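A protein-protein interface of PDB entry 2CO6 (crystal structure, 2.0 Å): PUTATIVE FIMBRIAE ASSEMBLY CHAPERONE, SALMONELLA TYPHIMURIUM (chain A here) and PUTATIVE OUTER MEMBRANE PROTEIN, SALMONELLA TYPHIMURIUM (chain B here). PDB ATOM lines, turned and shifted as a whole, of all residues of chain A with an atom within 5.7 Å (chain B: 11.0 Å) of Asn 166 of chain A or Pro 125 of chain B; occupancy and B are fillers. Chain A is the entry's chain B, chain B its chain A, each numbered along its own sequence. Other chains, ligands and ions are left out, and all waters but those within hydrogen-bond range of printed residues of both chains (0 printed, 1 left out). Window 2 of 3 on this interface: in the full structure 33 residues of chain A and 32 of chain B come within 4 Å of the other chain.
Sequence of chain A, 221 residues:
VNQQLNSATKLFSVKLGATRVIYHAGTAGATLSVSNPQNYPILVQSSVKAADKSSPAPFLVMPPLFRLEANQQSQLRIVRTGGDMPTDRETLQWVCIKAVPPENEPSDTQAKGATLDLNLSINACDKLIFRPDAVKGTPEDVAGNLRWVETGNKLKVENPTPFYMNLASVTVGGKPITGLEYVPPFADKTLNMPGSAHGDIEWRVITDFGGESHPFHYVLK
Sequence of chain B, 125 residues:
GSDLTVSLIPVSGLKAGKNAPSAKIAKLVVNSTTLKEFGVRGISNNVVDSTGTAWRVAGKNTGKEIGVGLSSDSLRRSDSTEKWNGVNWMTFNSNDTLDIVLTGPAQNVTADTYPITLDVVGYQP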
ATOM      1  N   THR A  19      -8.853  -7.189 -29.676  1.00  0.00           N
ATOM      2  CA  THR A  19      -8.950  -8.516 -29.036  1.00  0.00           C
ATOM      3  C   THR A  19     -10.337  -9.174 -29.192  1.00  0.00           C
ATOM      4  O   THR A  19     -10.512 -10.345 -28.894  1.00  0.00           O
ATOM      5  CB  THR A  19      -8.638  -8.443 -27.554  1.00  0.00           C
ATOM      6  OG1 THR A  19      -9.606  -7.583 -26.900  1.00  0.00           O
ATOM      7  CG2 THR A  19      -7.200  -7.911 -27.354  1.00  0.00           C
ATOM      8  N   ARG A  20     -11.320  -8.405 -29.638  1.00  0.00           N
ATOM      9  CA  ARG A  20     -12.604  -8.968 -30.036  1.00  0.00           C
ATOM     10  C   ARG A  20     -13.107  -8.142 -31.171  1.00  0.00           C
ATOM     11  O   ARG A  20     -12.621  -7.038 -31.417  1.00  0.00           O
ATOM     12  CB  ARG A  20     -13.630  -8.942 -28.886  1.00  0.00           C
ATOM     13  CG  ARG A  20     -13.992  -7.496 -28.396  1.00  0.00           C
ATOM     14  CD  ARG A  20     -13.292  -7.153 -27.132  1.00  0.00           C
ATOM     15  NE  ARG A  20     -13.804  -8.072 -26.126  1.00  0.00           N
ATOM     16  CZ  ARG A  20     -13.114  -9.064 -25.580  1.00  0.00           C
ATOM     17  NH1 ARG A  20     -11.818  -9.226 -25.874  1.00  0.00           N
ATOM     18  NH2 ARG A  20     -13.731  -9.886 -24.720  1.00  0.00           N
ATOM     19  N   LEU A  92     -21.787 -16.232 -30.337  1.00  0.00           N
ATOM     20  CA  LEU A  92     -20.327 -16.213 -30.347  1.00  0.00           C
ATOM     21  C   LEU A  92     -19.658 -17.177 -31.356  1.00  0.00           C
ATOM     22  O   LEU A  92     -20.020 -18.354 -31.480  1.00  0.00           O
ATOM     23  CB  LEU A  92     -19.779 -16.482 -28.948  1.00  0.00           C
ATOM     24  CG  LEU A  92     -18.255 -16.266 -28.858  1.00  0.00           C
ATOM     25  CD1 LEU A  92     -17.994 -15.541 -27.581  1.00  0.00           C
ATOM     26  CD2 LEU A  92     -17.511 -17.593 -28.870  1.00  0.00           C
ATOM     27  N   TRP A  94     -15.402 -17.554 -33.263  1.00  0.00           N
ATOM     28  CA  TRP A  94     -13.999 -17.188 -33.139  1.00  0.00           C
ATOM     29  C   TRP A  94     -13.400 -16.851 -34.521  1.00  0.00           C
ATOM     30  O   TRP A  94     -13.504 -17.634 -35.434  1.00  0.00           O
ATOM     31  CB  TRP A  94     -13.231 -18.350 -32.504  1.00  0.00           C
ATOM     32  CG  TRP A  94     -13.576 -18.636 -31.044  1.00  0.00           C
ATOM     33  CD1 TRP A  94     -14.444 -19.577 -30.559  1.00  0.00           C
ATOM     34  CD2 TRP A  94     -13.015 -17.981 -29.892  1.00  0.00           C
ATOM     35  NE1 TRP A  94     -14.419 -19.585 -29.161  1.00  0.00           N
ATOM     36  CE2 TRP A  94     -13.587 -18.585 -28.736  1.00  0.00           C
ATOM     37  CE3 TRP A  94     -12.067 -16.950 -29.725  1.00  0.00           C
ATOM     38  CZ2 TRP A  94     -13.249 -18.181 -27.421  1.00  0.00           C
ATOM     39  CZ3 TRP A  94     -11.737 -16.556 -28.434  1.00  0.00           C
ATOM     40  CH2 TRP A  94     -12.331 -17.171 -27.296  1.00  0.00           C
ATOM     41  N   LYS A 127     -12.693 -13.373 -30.178  1.00  0.00           N
ATOM     42  CA  LYS A 127     -14.124 -13.546 -30.234  1.00  0.00           C
ATOM     43  C   LYS A 127     -14.731 -12.620 -31.328  1.00  0.00           C
ATOM     44  O   LYS A 127     -14.451 -11.424 -31.390  1.00  0.00           O
ATOM     45  CB  LYS A 127     -14.760 -13.285 -28.871  1.00  0.00           C
ATOM     46  CG  LYS A 127     -14.275 -14.269 -27.796  1.00  0.00           C
ATOM     47  CD  LYS A 127     -14.766 -13.931 -26.402  1.00  0.00           C
ATOM     48  CE  LYS A 127     -14.207 -14.961 -25.415  1.00  0.00           C
ATOM     49  NZ  LYS A 127     -14.159 -14.440 -24.074  1.00  0.00           N
ATOM     50  N   ILE A 129     -18.328 -11.650 -32.065  1.00  0.00           N
ATOM     51  CA  ILE A 129     -19.630 -11.716 -31.409  1.00  0.00           C
ATOM     52  C   ILE A 129     -20.719 -11.062 -32.265  1.00  0.00           C
ATOM     53  O   ILE A 129     -20.691  -9.859 -32.538  1.00  0.00           O
ATOM     54  CB  ILE A 129     -19.591 -11.084 -30.012  1.00  0.00           C
ATOM     55  CG1 ILE A 129     -18.499 -11.782 -29.166  1.00  0.00           C
ATOM     56  CG2 ILE A 129     -20.995 -11.202 -29.356  1.00  0.00           C
ATOM     57  CD1 ILE A 129     -18.295 -11.204 -27.775  1.00  0.00           C
ATOM     58  N   TYR A 164     -23.072 -12.223 -24.276  1.00  0.00           N
ATOM     59  CA  TYR A 164     -21.925 -12.914 -23.703  1.00  0.00           C
ATOM     60  C   TYR A 164     -21.249 -11.993 -22.695  1.00  0.00           C
ATOM     61  O   TYR A 164     -20.984 -10.806 -22.947  1.00  0.00           O
ATOM     62  CB  TYR A 164     -20.925 -13.385 -24.770  1.00  0.00           C
ATOM     63  CG  TYR A 164     -21.446 -14.518 -25.575  1.00  0.00           C
ATOM     64  CD1 TYR A 164     -21.149 -15.846 -25.241  1.00  0.00           C
ATOM     65  CD2 TYR A 164     -22.266 -14.274 -26.678  1.00  0.00           C
ATOM     66  CE1 TYR A 164     -21.644 -16.909 -26.008  1.00  0.00           C
ATOM     67  CE2 TYR A 164     -22.768 -15.300 -27.424  1.00  0.00           C
ATOM     68  CZ  TYR A 164     -22.477 -16.614 -27.085  1.00  0.00           C
ATOM     69  OH  TYR A 164     -23.005 -17.593 -27.887  1.00  0.00           O
ATOM     70  N   MET A 165     -21.006 -12.532 -21.526  1.00  0.00           N
ATOM     71  CA  MET A 165     -20.326 -11.785 -20.513  1.00  0.00           C
ATOM     72  C   MET A 165     -18.930 -12.333 -20.436  1.00  0.00           C
ATOM     73  O   MET A 165     -18.705 -13.470 -19.983  1.00  0.00           O
ATOM     74  CB  MET A 165     -21.045 -11.889 -19.162  1.00  0.00           C
ATOM     75  CG  MET A 165     -22.396 -11.197 -19.159  1.00  0.00           C
ATOM     76  SD  MET A 165     -22.139  -9.418 -19.053  1.00  0.00           S
ATOM     77  CE  MET A 165     -23.826  -8.826 -19.334  1.00  0.00           C
ATOM     78  N   ASN A 166     -17.996 -11.497 -20.898  1.00  0.00           N
ATOM     79  CA  ASN A 166     -16.618 -11.866 -21.022  1.00  0.00           C
ATOM     80  C   ASN A 166     -15.887 -11.271 -19.820  1.00  0.00           C
ATOM     81  O   ASN A 166     -15.456 -10.116 -19.820  1.00  0.00           O
ATOM     82  CB  ASN A 166     -16.058 -11.374 -22.352  1.00  0.00           C
ATOM     83  CG  ASN A 166     -16.860 -11.895 -23.520  1.00  0.00           C
ATOM     84  OD1 ASN A 166     -16.841 -13.071 -23.799  1.00  0.00           O
ATOM     85  ND2 ASN A 166     -17.603 -11.023 -24.176  1.00  0.00           N
ATOM     86  N   LEU A 167     -15.775 -12.105 -18.805  1.00  0.00           N
ATOM     87  CA  LEU A 167     -15.234 -11.746 -17.506  1.00  0.00           C
ATOM     88  C   LEU A 167     -13.754 -11.472 -17.663  1.00  0.00           C
ATOM     89  O   LEU A 167     -13.059 -12.252 -18.299  1.00  0.00           O
ATOM     90  CB  LEU A 167     -15.446 -12.913 -16.533  1.00  0.00           C
ATOM     91  CG  LEU A 167     -16.668 -12.998 -15.591  1.00  0.00           C
ATOM     92  CD1 LEU A 167     -17.703 -11.904 -15.749  1.00  0.00           C
ATOM     93  CD2 LEU A 167     -17.264 -14.409 -15.611  1.00  0.00           C
ATOM     94  N   ALA A 168     -13.306 -10.342 -17.111  1.00  0.00           N
ATOM     95  CA  ALA A 168     -11.909  -9.935 -17.100  1.00  0.00           C
ATOM     96  C   ALA A 168     -11.362 -10.421 -15.769  1.00  0.00           C
ATOM     97  O   ALA A 168     -10.179 -10.782 -15.641  1.00  0.00           O
ATOM     98  CB  ALA A 168     -11.810  -8.410 -17.206  1.00  0.00           C
ATOM     99  N   TYR A 182     -16.231 -17.231 -20.446  1.00  0.00           N
ATOM    100  CA  TYR A 182     -17.352 -16.346 -20.727  1.00  0.00           C
ATOM    101  C   TYR A 182     -18.680 -16.977 -20.258  1.00  0.00           C
ATOM    102  O   TYR A 182     -18.798 -18.228 -20.210  1.00  0.00           O
ATOM    103  CB  TYR A 182     -17.430 -15.994 -22.205  1.00  0.00           C
ATOM    104  CG  TYR A 182     -17.535 -17.166 -23.175  1.00  0.00           C
ATOM    105  CD1 TYR A 182     -16.407 -17.636 -23.858  1.00  0.00           C
ATOM    106  CD2 TYR A 182     -18.779 -17.756 -23.464  1.00  0.00           C
ATOM    107  CE1 TYR A 182     -16.497 -18.694 -24.744  1.00  0.00           C
ATOM    108  CE2 TYR A 182     -18.889 -18.794 -24.357  1.00  0.00           C
ATOM    109  CZ  TYR A 182     -17.750 -19.259 -24.993  1.00  0.00           C
ATOM    110  OH  TYR A 182     -17.866 -20.295 -25.859  1.00  0.00           O
ATOM    111  N   VAL A 183     -19.650 -16.122 -19.914  1.00  0.00           N
ATOM    112  CA  VAL A 183     -20.996 -16.586 -19.585  1.00  0.00           C
ATOM    113  C   VAL A 183     -21.888 -16.273 -20.774  1.00  0.00           C
ATOM    114  O   VAL A 183     -22.032 -15.092 -21.155  1.00  0.00           O
ATOM    115  CB  VAL A 183     -21.581 -15.951 -18.313  1.00  0.00           C
ATOM    116  CG1 VAL A 183     -22.718 -16.851 -17.759  1.00  0.00           C
ATOM    117  CG2 VAL A 183     -20.491 -15.728 -17.254  1.00  0.00           C
ATOM    118  N   ARG A 204     -15.321  -7.766 -13.123  1.00  0.00           N
ATOM    119  CA  ARG A 204     -15.171  -6.827 -14.249  1.00  0.00           C
ATOM    120  C   ARG A 204     -15.480  -7.617 -15.507  1.00  0.00           C
ATOM    121  O   ARG A 204     -15.236  -8.837 -15.545  1.00  0.00           O
ATOM    122  CB  ARG A 204     -13.739  -6.289 -14.307  1.00  0.00           C
ATOM    123  CG  ARG A 204     -13.397  -5.298 -13.172  1.00  0.00           C
ATOM    124  CD  ARG A 204     -11.922  -4.798 -13.211  1.00  0.00           C
ATOM    125  NE  ARG A 204     -11.591  -3.993 -12.023  1.00  0.00           N
ATOM    126  CZ  ARG A 204     -11.441  -2.668 -12.018  1.00  0.00           C
ATOM    127  NH1 ARG A 204     -11.564  -1.958 -13.147  1.00  0.00           N
ATOM    128  NH2 ARG A 204     -11.155  -2.037 -10.875  1.00  0.00           N
ATOM    129  N   VAL A 205     -16.036  -6.968 -16.528  1.00  0.00           N
ATOM    130  CA  VAL A 205     -16.070  -7.603 -17.850  1.00  0.00           C
ATOM    131  C   VAL A 205     -15.172  -6.850 -18.845  1.00  0.00           C
ATOM    132  O   VAL A 205     -14.881  -5.660 -18.652  1.00  0.00           O
ATOM    133  CB  VAL A 205     -17.478  -7.709 -18.466  1.00  0.00           C
ATOM    134  CG1 VAL A 205     -18.387  -8.638 -17.641  1.00  0.00           C
ATOM    135  CG2 VAL A 205     -18.090  -6.354 -18.666  1.00  0.00           C
ATOM    136  N   ILE A 206     -14.769  -7.538 -19.913  1.00  0.00           N
ATOM    137  CA  ILE A 206     -14.028  -6.906 -20.992  1.00  0.00           C
ATOM    138  C   ILE A 206     -15.105  -6.264 -21.858  1.00  0.00           C
ATOM    139  O   ILE A 206     -16.100  -6.902 -22.195  1.00  0.00           O
ATOM    140  CB  ILE A 206     -13.197  -7.927 -21.798  1.00  0.00           C
ATOM    141  CG1 ILE A 206     -12.280  -8.706 -20.838  1.00  0.00           C
ATOM    142  CG2 ILE A 206     -12.377  -7.212 -22.819  1.00  0.00           C
ATOM    143  CD1 ILE A 206     -11.311  -9.660 -21.489  1.00  0.00           C
ATOM    144  N   THR A 207     -14.939  -4.981 -22.164  1.00  0.00           N
ATOM    145  CA  THR A 207     -15.959  -4.259 -22.951  1.00  0.00           C
ATOM    146  C   THR A 207     -15.832  -4.585 -24.424  1.00  0.00           C
ATOM    147  O   THR A 207     -14.889  -5.258 -24.829  1.00  0.00           O
ATOM    148  CB  THR A 207     -15.799  -2.724 -22.782  1.00  0.00           C
ATOM    149  OG1 THR A 207     -14.619  -2.297 -23.475  1.00  0.00           O
ATOM    150  CG2 THR A 207     -15.704  -2.339 -21.309  1.00  0.00           C
ATOM    151  N   GLY B   1       4.141  -6.321 -25.533  1.00  0.00           N
ATOM    152  CA  GLY B   1       3.276  -7.200 -24.704  1.00  0.00           C
ATOM    153  C   GLY B   1       1.875  -7.335 -25.304  1.00  0.00           C
ATOM    154  O   GLY B   1       1.251  -8.409 -25.232  1.00  0.00           O
ATOM    155  N   SER B   2       1.375  -6.236 -25.844  1.00  0.00           N
ATOM    156  CA  SER B   2       0.082  -6.194 -26.513  1.00  0.00           C
ATOM    157  C   SER B   2      -0.103  -7.441 -27.401  1.00  0.00           C
ATOM    158  O   SER B   2      -1.108  -8.159 -27.290  1.00  0.00           O
ATOM    159  CB  SER B   2       0.026  -4.916 -27.361  1.00  0.00           C
ATOM    160  OG  SER B   2      -1.256  -4.756 -27.963  1.00  0.00           O
ATOM    161  N   LEU B   4       0.564 -11.111 -29.501  1.00  0.00           N
ATOM    162  CA  LEU B   4       1.058 -12.498 -29.414  1.00  0.00           C
ATOM    163  C   LEU B   4       2.483 -12.636 -29.964  1.00  0.00           C
ATOM    164  O   LEU B   4       2.715 -12.430 -31.167  1.00  0.00           O
ATOM    165  CB  LEU B   4       0.143 -13.459 -30.167  1.00  0.00           C
ATOM    166  CG  LEU B   4      -0.087 -14.869 -29.615  1.00  0.00           C
ATOM    167  CD1 LEU B   4      -0.086 -15.881 -30.767  1.00  0.00           C
ATOM    168  CD2 LEU B   4       0.849 -15.278 -28.451  1.00  0.00           C
ATOM    169  N   SER B  32       2.172 -12.475 -24.077  1.00  0.00           N
ATOM    170  CA  SER B  32       1.043 -11.607 -24.420  1.00  0.00           C
ATOM    171  C   SER B  32       0.505 -11.045 -23.108  1.00  0.00           C
ATOM    172  O   SER B  32       0.407 -11.761 -22.107  1.00  0.00           O
ATOM    173  CB  SER B  32      -0.040 -12.406 -25.153  1.00  0.00           C
ATOM    174  OG  SER B  32      -1.300 -11.743 -25.153  1.00  0.00           O
ATOM    175  N   THR B  33       0.150  -9.769 -23.085  1.00  0.00           N
ATOM    176  CA  THR B  33      -0.322  -9.183 -21.814  1.00  0.00           C
ATOM    177  C   THR B  33      -1.784  -9.454 -21.584  1.00  0.00           C
ATOM    178  O   THR B  33      -2.293  -9.190 -20.507  1.00  0.00           O
ATOM    179  CB  THR B  33      -0.097  -7.686 -21.749  1.00  0.00           C
ATOM    180  OG1 THR B  33      -0.702  -7.072 -22.898  1.00  0.00           O
ATOM    181  CG2 THR B  33       1.404  -7.399 -21.702  1.00  0.00           C
ATOM    182  N   THR B  34      -2.469  -9.966 -22.593  1.00  0.00           N
ATOM    183  CA  THR B  34      -3.898 -10.259 -22.460  1.00  0.00           C
ATOM    184  C   THR B  34      -4.271 -11.744 -22.370  1.00  0.00           C
ATOM    185  O   THR B  34      -5.289 -12.073 -21.791  1.00  0.00           O
ATOM    186  CB  THR B  34      -4.708  -9.588 -23.589  1.00  0.00           C
ATOM    187  OG1 THR B  34      -4.075  -9.858 -24.847  1.00  0.00           O
ATOM    188  CG2 THR B  34      -4.790  -8.064 -23.352  1.00  0.00           C
ATOM    189  N   LEU B  35      -3.435 -12.631 -22.910  1.00  0.00           N
ATOM    190  CA  LEU B  35      -3.679 -14.071 -22.887  1.00  0.00           C
ATOM    191  C   LEU B  35      -3.530 -14.687 -21.496  1.00  0.00           C
ATOM    192  O   LEU B  35      -2.677 -14.273 -20.710  1.00  0.00           O
ATOM    193  CB  LEU B  35      -2.713 -14.784 -23.833  1.00  0.00           C
ATOM    194  CG  LEU B  35      -3.020 -15.033 -25.295  1.00  0.00           C
ATOM    195  CD1 LEU B  35      -1.911 -15.910 -25.875  1.00  0.00           C
ATOM    196  CD2 LEU B  35      -4.379 -15.696 -25.467  1.00  0.00           C
ATOM    197  N   LYS B  36      -4.343 -15.695 -21.210  1.00  0.00           N
ATOM    198  CA  LYS B  36      -4.281 -16.412 -19.944  1.00  0.00           C
ATOM    199  C   LYS B  36      -3.738 -17.825 -20.170  1.00  0.00           C
ATOM    200  O   LYS B  36      -3.011 -18.369 -19.337  1.00  0.00           O
ATOM    201  CB  LYS B  36      -5.663 -16.451 -19.255  1.00  0.00           C
ATOM    202  CG  LYS B  36      -6.259 -15.091 -18.971  1.00  0.00           C
ATOM    203  CD  LYS B  36      -5.364 -14.281 -18.031  1.00  0.00           C
ATOM    204  CE  LYS B  36      -5.727 -12.778 -18.042  1.00  0.00           C
ATOM    205  NZ  LYS B  36      -6.912 -12.518 -17.209  1.00  0.00           N
ATOM    206  N   GLU B  37      -4.061 -18.403 -21.319  1.00  0.00           N
ATOM    207  CA  GLU B  37      -3.533 -19.722 -21.630  1.00  0.00           C
ATOM    208  C   GLU B  37      -3.202 -19.858 -23.111  1.00  0.00           C
ATOM    209  O   GLU B  37      -3.637 -19.046 -23.913  1.00  0.00           O
ATOM    210  CB  GLU B  37      -4.515 -20.810 -21.147  1.00  0.00           C
ATOM    211  CG  GLU B  37      -5.395 -21.415 -22.192  1.00  0.00           C
ATOM    212  CD  GLU B  37      -6.480 -22.307 -21.595  1.00  0.00           C
ATOM    213  OE1 GLU B  37      -7.504 -22.493 -22.283  1.00  0.00           O
ATOM    214  OE2 GLU B  37      -6.304 -22.818 -20.448  1.00  0.00           O
ATOM    215  N   PHE B  38      -2.412 -20.866 -23.460  1.00  0.00           N
ATOM    216  CA  PHE B  38      -2.153 -21.188 -24.875  1.00  0.00           C
ATOM    217  C   PHE B  38      -2.151 -22.701 -25.045  1.00  0.00           C
ATOM    218  O   PHE B  38      -2.031 -23.442 -24.070  1.00  0.00           O
ATOM    219  CB  PHE B  38      -0.826 -20.585 -25.365  1.00  0.00           C
ATOM    220  CG  PHE B  38       0.403 -21.189 -24.711  1.00  0.00           C
ATOM    221  CD1 PHE B  38       1.086 -22.237 -25.318  1.00  0.00           C
ATOM    222  CD2 PHE B  38       0.894 -20.676 -23.512  1.00  0.00           C
ATOM    223  CE1 PHE B  38       2.244 -22.809 -24.709  1.00  0.00           C
ATOM    224  CE2 PHE B  38       2.037 -21.210 -22.890  1.00  0.00           C
ATOM    225  CZ  PHE B  38       2.730 -22.280 -23.501  1.00  0.00           C
ATOM    226  N   TRP B  84      -9.715 -28.708 -30.369  1.00  0.00           N
ATOM    227  CA  TRP B  84      -9.816 -27.477 -31.113  1.00  0.00           C
ATOM    228  C   TRP B  84      -9.464 -27.849 -32.518  1.00  0.00           C
ATOM    229  O   TRP B  84      -8.462 -28.515 -32.742  1.00  0.00           O
ATOM    230  CB  TRP B  84      -8.775 -26.479 -30.605  1.00  0.00           C
ATOM    231  CG  TRP B  84      -8.981 -25.937 -29.215  1.00  0.00           C
ATOM    232  CD1 TRP B  84     -10.141 -25.920 -28.481  1.00  0.00           C
ATOM    233  CD2 TRP B  84      -7.986 -25.300 -28.409  1.00  0.00           C
ATOM    234  NE1 TRP B  84      -9.915 -25.299 -27.270  1.00  0.00           N
ATOM    235  CE2 TRP B  84      -8.602 -24.910 -27.207  1.00  0.00           C
ATOM    236  CE3 TRP B  84      -6.628 -25.000 -28.602  1.00  0.00           C
ATOM    237  CZ2 TRP B  84      -7.909 -24.246 -26.181  1.00  0.00           C
ATOM    238  CZ3 TRP B  84      -5.941 -24.329 -27.586  1.00  0.00           C
ATOM    239  CH2 TRP B  84      -6.587 -23.957 -26.394  1.00  0.00           C
ATOM    240  N   PHE B  92      -1.801 -24.629 -21.645  1.00  0.00           N
ATOM    241  CA  PHE B  92      -0.826 -24.192 -20.670  1.00  0.00           C
ATOM    242  C   PHE B  92      -1.099 -22.780 -20.257  1.00  0.00           C
ATOM    243  O   PHE B  92      -1.585 -21.957 -21.043  1.00  0.00           O
ATOM    244  CB  PHE B  92       0.596 -24.284 -21.250  1.00  0.00           C
ATOM    245  CG  PHE B  92       0.971 -25.667 -21.648  1.00  0.00           C
ATOM    246  CD1 PHE B  92       0.672 -26.135 -22.911  1.00  0.00           C
ATOM    247  CD2 PHE B  92       1.549 -26.531 -20.721  1.00  0.00           C
ATOM    248  CE1 PHE B  92       0.980 -27.430 -23.273  1.00  0.00           C
ATOM    249  CE2 PHE B  92       1.852 -27.816 -21.074  1.00  0.00           C
ATOM    250  CZ  PHE B  92       1.577 -28.271 -22.347  1.00  0.00           C
ATOM    251  N   SER B  94      -0.178 -19.171 -19.791  1.00  0.00           N
ATOM    252  CA  SER B  94       0.647 -18.314 -20.639  1.00  0.00           C
ATOM    253  C   SER B  94       1.886 -17.756 -19.927  1.00  0.00           C
ATOM    254  O   SER B  94       2.775 -17.196 -20.578  1.00  0.00           O
ATOM    255  CB  SER B  94      -0.196 -17.210 -21.303  1.00  0.00           C
ATOM    256  OG  SER B  94      -0.823 -16.360 -20.355  1.00  0.00           O
ATOM    257  N   VAL B 121      -1.394 -21.588 -30.385  1.00  0.00           N
ATOM    258  CA  VAL B 121      -2.691 -20.938 -30.443  1.00  0.00           C
ATOM    259  C   VAL B 121      -3.016 -20.225 -29.124  1.00  0.00           C
ATOM    260  O   VAL B 121      -2.839 -20.778 -27.987  1.00  0.00           O
ATOM    261  CB  VAL B 121      -3.799 -21.976 -30.825  1.00  0.00           C
ATOM    262  CG1 VAL B 121      -3.852 -23.051 -29.824  1.00  0.00           C
ATOM    263  CG2 VAL B 121      -5.190 -21.320 -30.913  1.00  0.00           C
ATOM    264  N   GLY B 122      -3.484 -18.983 -29.258  1.00  0.00           N
ATOM    265  CA  GLY B 122      -4.044 -18.263 -28.114  1.00  0.00           C
ATOM    266  C   GLY B 122      -5.429 -17.757 -28.427  1.00  0.00           C
ATOM    267  O   GLY B 122      -5.618 -17.017 -29.405  1.00  0.00           O
ATOM    268  N   TYR B 123      -6.397 -18.184 -27.627  1.00  0.00           N
ATOM    269  CA  TYR B 123      -7.766 -17.642 -27.632  1.00  0.00           C
ATOM    270  C   TYR B 123      -7.914 -16.475 -26.648  1.00  0.00           C
ATOM    271  O   TYR B 123      -7.791 -16.650 -25.409  1.00  0.00           O
ATOM    272  CB  TYR B 123      -8.746 -18.746 -27.255  1.00  0.00           C
ATOM    273  CG  TYR B 123      -8.837 -19.804 -28.312  1.00  0.00           C
ATOM    274  CD1 TYR B 123      -8.040 -20.958 -28.243  1.00  0.00           C
ATOM    275  CD2 TYR B 123      -9.678 -19.621 -29.427  1.00  0.00           C
ATOM    276  CE1 TYR B 123      -8.113 -21.921 -29.238  1.00  0.00           C
ATOM    277  CE2 TYR B 123      -9.755 -20.572 -30.432  1.00  0.00           C
ATOM    278  CZ  TYR B 123      -8.991 -21.714 -30.337  1.00  0.00           C
ATOM    279  OH  TYR B 123      -9.078 -22.657 -31.341  1.00  0.00           O
ATOM    280  N   GLN B 124      -8.174 -15.283 -27.194  1.00  0.00           N
ATOM    281  CA  GLN B 124      -8.245 -14.081 -26.367  1.00  0.00           C
ATOM    282  C   GLN B 124      -9.509 -14.102 -25.514  1.00  0.00           C
ATOM    283  O   GLN B 124     -10.608 -14.403 -25.997  1.00  0.00           O
ATOM    284  CB  GLN B 124      -8.213 -12.787 -27.201  1.00  0.00           C
ATOM    285  CG  GLN B 124      -6.856 -12.393 -27.772  1.00  0.00           C
ATOM    286  CD  GLN B 124      -5.864 -11.915 -26.702  1.00  0.00           C
ATOM    287  OE1 GLN B 124      -6.237 -11.219 -25.766  1.00  0.00           O
ATOM    288  NE2 GLN B 124      -4.596 -12.270 -26.862  1.00  0.00           N
ATOM    289  N   PRO B 125      -9.345 -13.805 -24.221  1.00  0.00           N
ATOM    290  CA  PRO B 125     -10.517 -13.523 -23.396  1.00  0.00           C
ATOM    291  C   PRO B 125     -11.286 -12.318 -23.896  1.00  0.00           C
ATOM    292  O   PRO B 125     -12.518 -12.267 -23.733  1.00  0.00           O
ATOM    293  CB  PRO B 125      -9.908 -13.261 -22.034  1.00  0.00           C
ATOM    294  CG  PRO B 125      -8.593 -14.066 -22.075  1.00  0.00           C
ATOM    295  CD  PRO B 125      -8.096 -13.787 -23.441  1.00  0.00           C
ATOM    296  OXT PRO B 125     -10.691 -11.384 -24.487  1.00  0.00           O
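The backbone carbonyl oxygen (O) of Thr 207 of chain A sits at hydrogen-bond distance from the guanidinium group (NE) of Arg 20 of chain A. NZ of Lys 127 of chain A lies within hydrogen-bond range of OD1 of Asn 166 of chain A, 3.0 Å away. The side-chain amide oxygen of Gln 124 of chain B is in hydrogen-bond range of the side-chain hydroxyl of Thr 34 of chain B (2.7 Å). NH1 of Arg 20 of chain A is in hydrogen-bond range of OG1 of Thr 19 of chain A. The backbone NH (N) of Ile 206 of chain A sits at hydrogen-bond distance from the backbone carbonyl oxygen (O) of Asn 166 of chain A.
The guanidinium group (NH1) of Arg 20 of chain A is in salt-bridge range of the chain-end carboxylate (OXT) of Pro 125 of chain B (2.8 Å). The chain-end carboxylate (O) of Pro 125 of chain B lies within salt-bridge range of the side-chain amino group (NZ) of Lys 127 of chain A (2.7 Å).
Of the printed residues of chain B, Arg 20 of chain A touches Pro 125. Of the printed residues of chain B, Lys 127 of chain A touches Gln 124 and Pro 125. No residue of chain B comes within 4 Å of Met 165 of chain A. Of chain B, only Pro 125 (3.9 Å) comes within 4 Å of Asn 166 of chain A. Leu 167 of chain A touches none of the printed residues of chain B. Printed residues of chain B within 4 Å of Ile 206 of chain A: Pro 125. Of the printed residues of chain A, Tyr 123 of chain B touches Trp 94. Of the printed residues of chain A, Gln 124 of chain B touches Thr 19, Trp 94 and Lys 127. Pro 125 of chain B touches just these residues of chain A: Arg 20, Lys 127, Asn 166 and Ile 206. The nearest residue of chain B that does not touch Asn 166 of chain A is Gln 124 of chain B (6.7 Å). The nearest printed residue of chain A that does not touch Tyr 123 of chain B is Lys 127 of chain A (6.6 Å).
Among the printed residues, merely in contact across the chains: Thr 19 of chain A with Gln 124 of chain B, Trp 94 of chain A with Tyr 123 of chain B, Trp 94 of chain A with Gln 124 of chain B, Lys 127 of chain A with Gln 124 of chain B, Asn 166 of chain A with Pro 125 of chain B and Ile 206 of chain A with Pro 125 of chain B.
Of the 18 printed residues of chain B, 3 touch a printed residue of chain A. Printed residues of chain B that touch a printed residue of chain A: Tyr 123, Gln 124 and Pro 125. Hydrophobic or aromatic side chains of chain B that line the printed part of chain A: Tyr 123 and Pro 125. Among the printed residues, 8 pairs touch across the chains.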
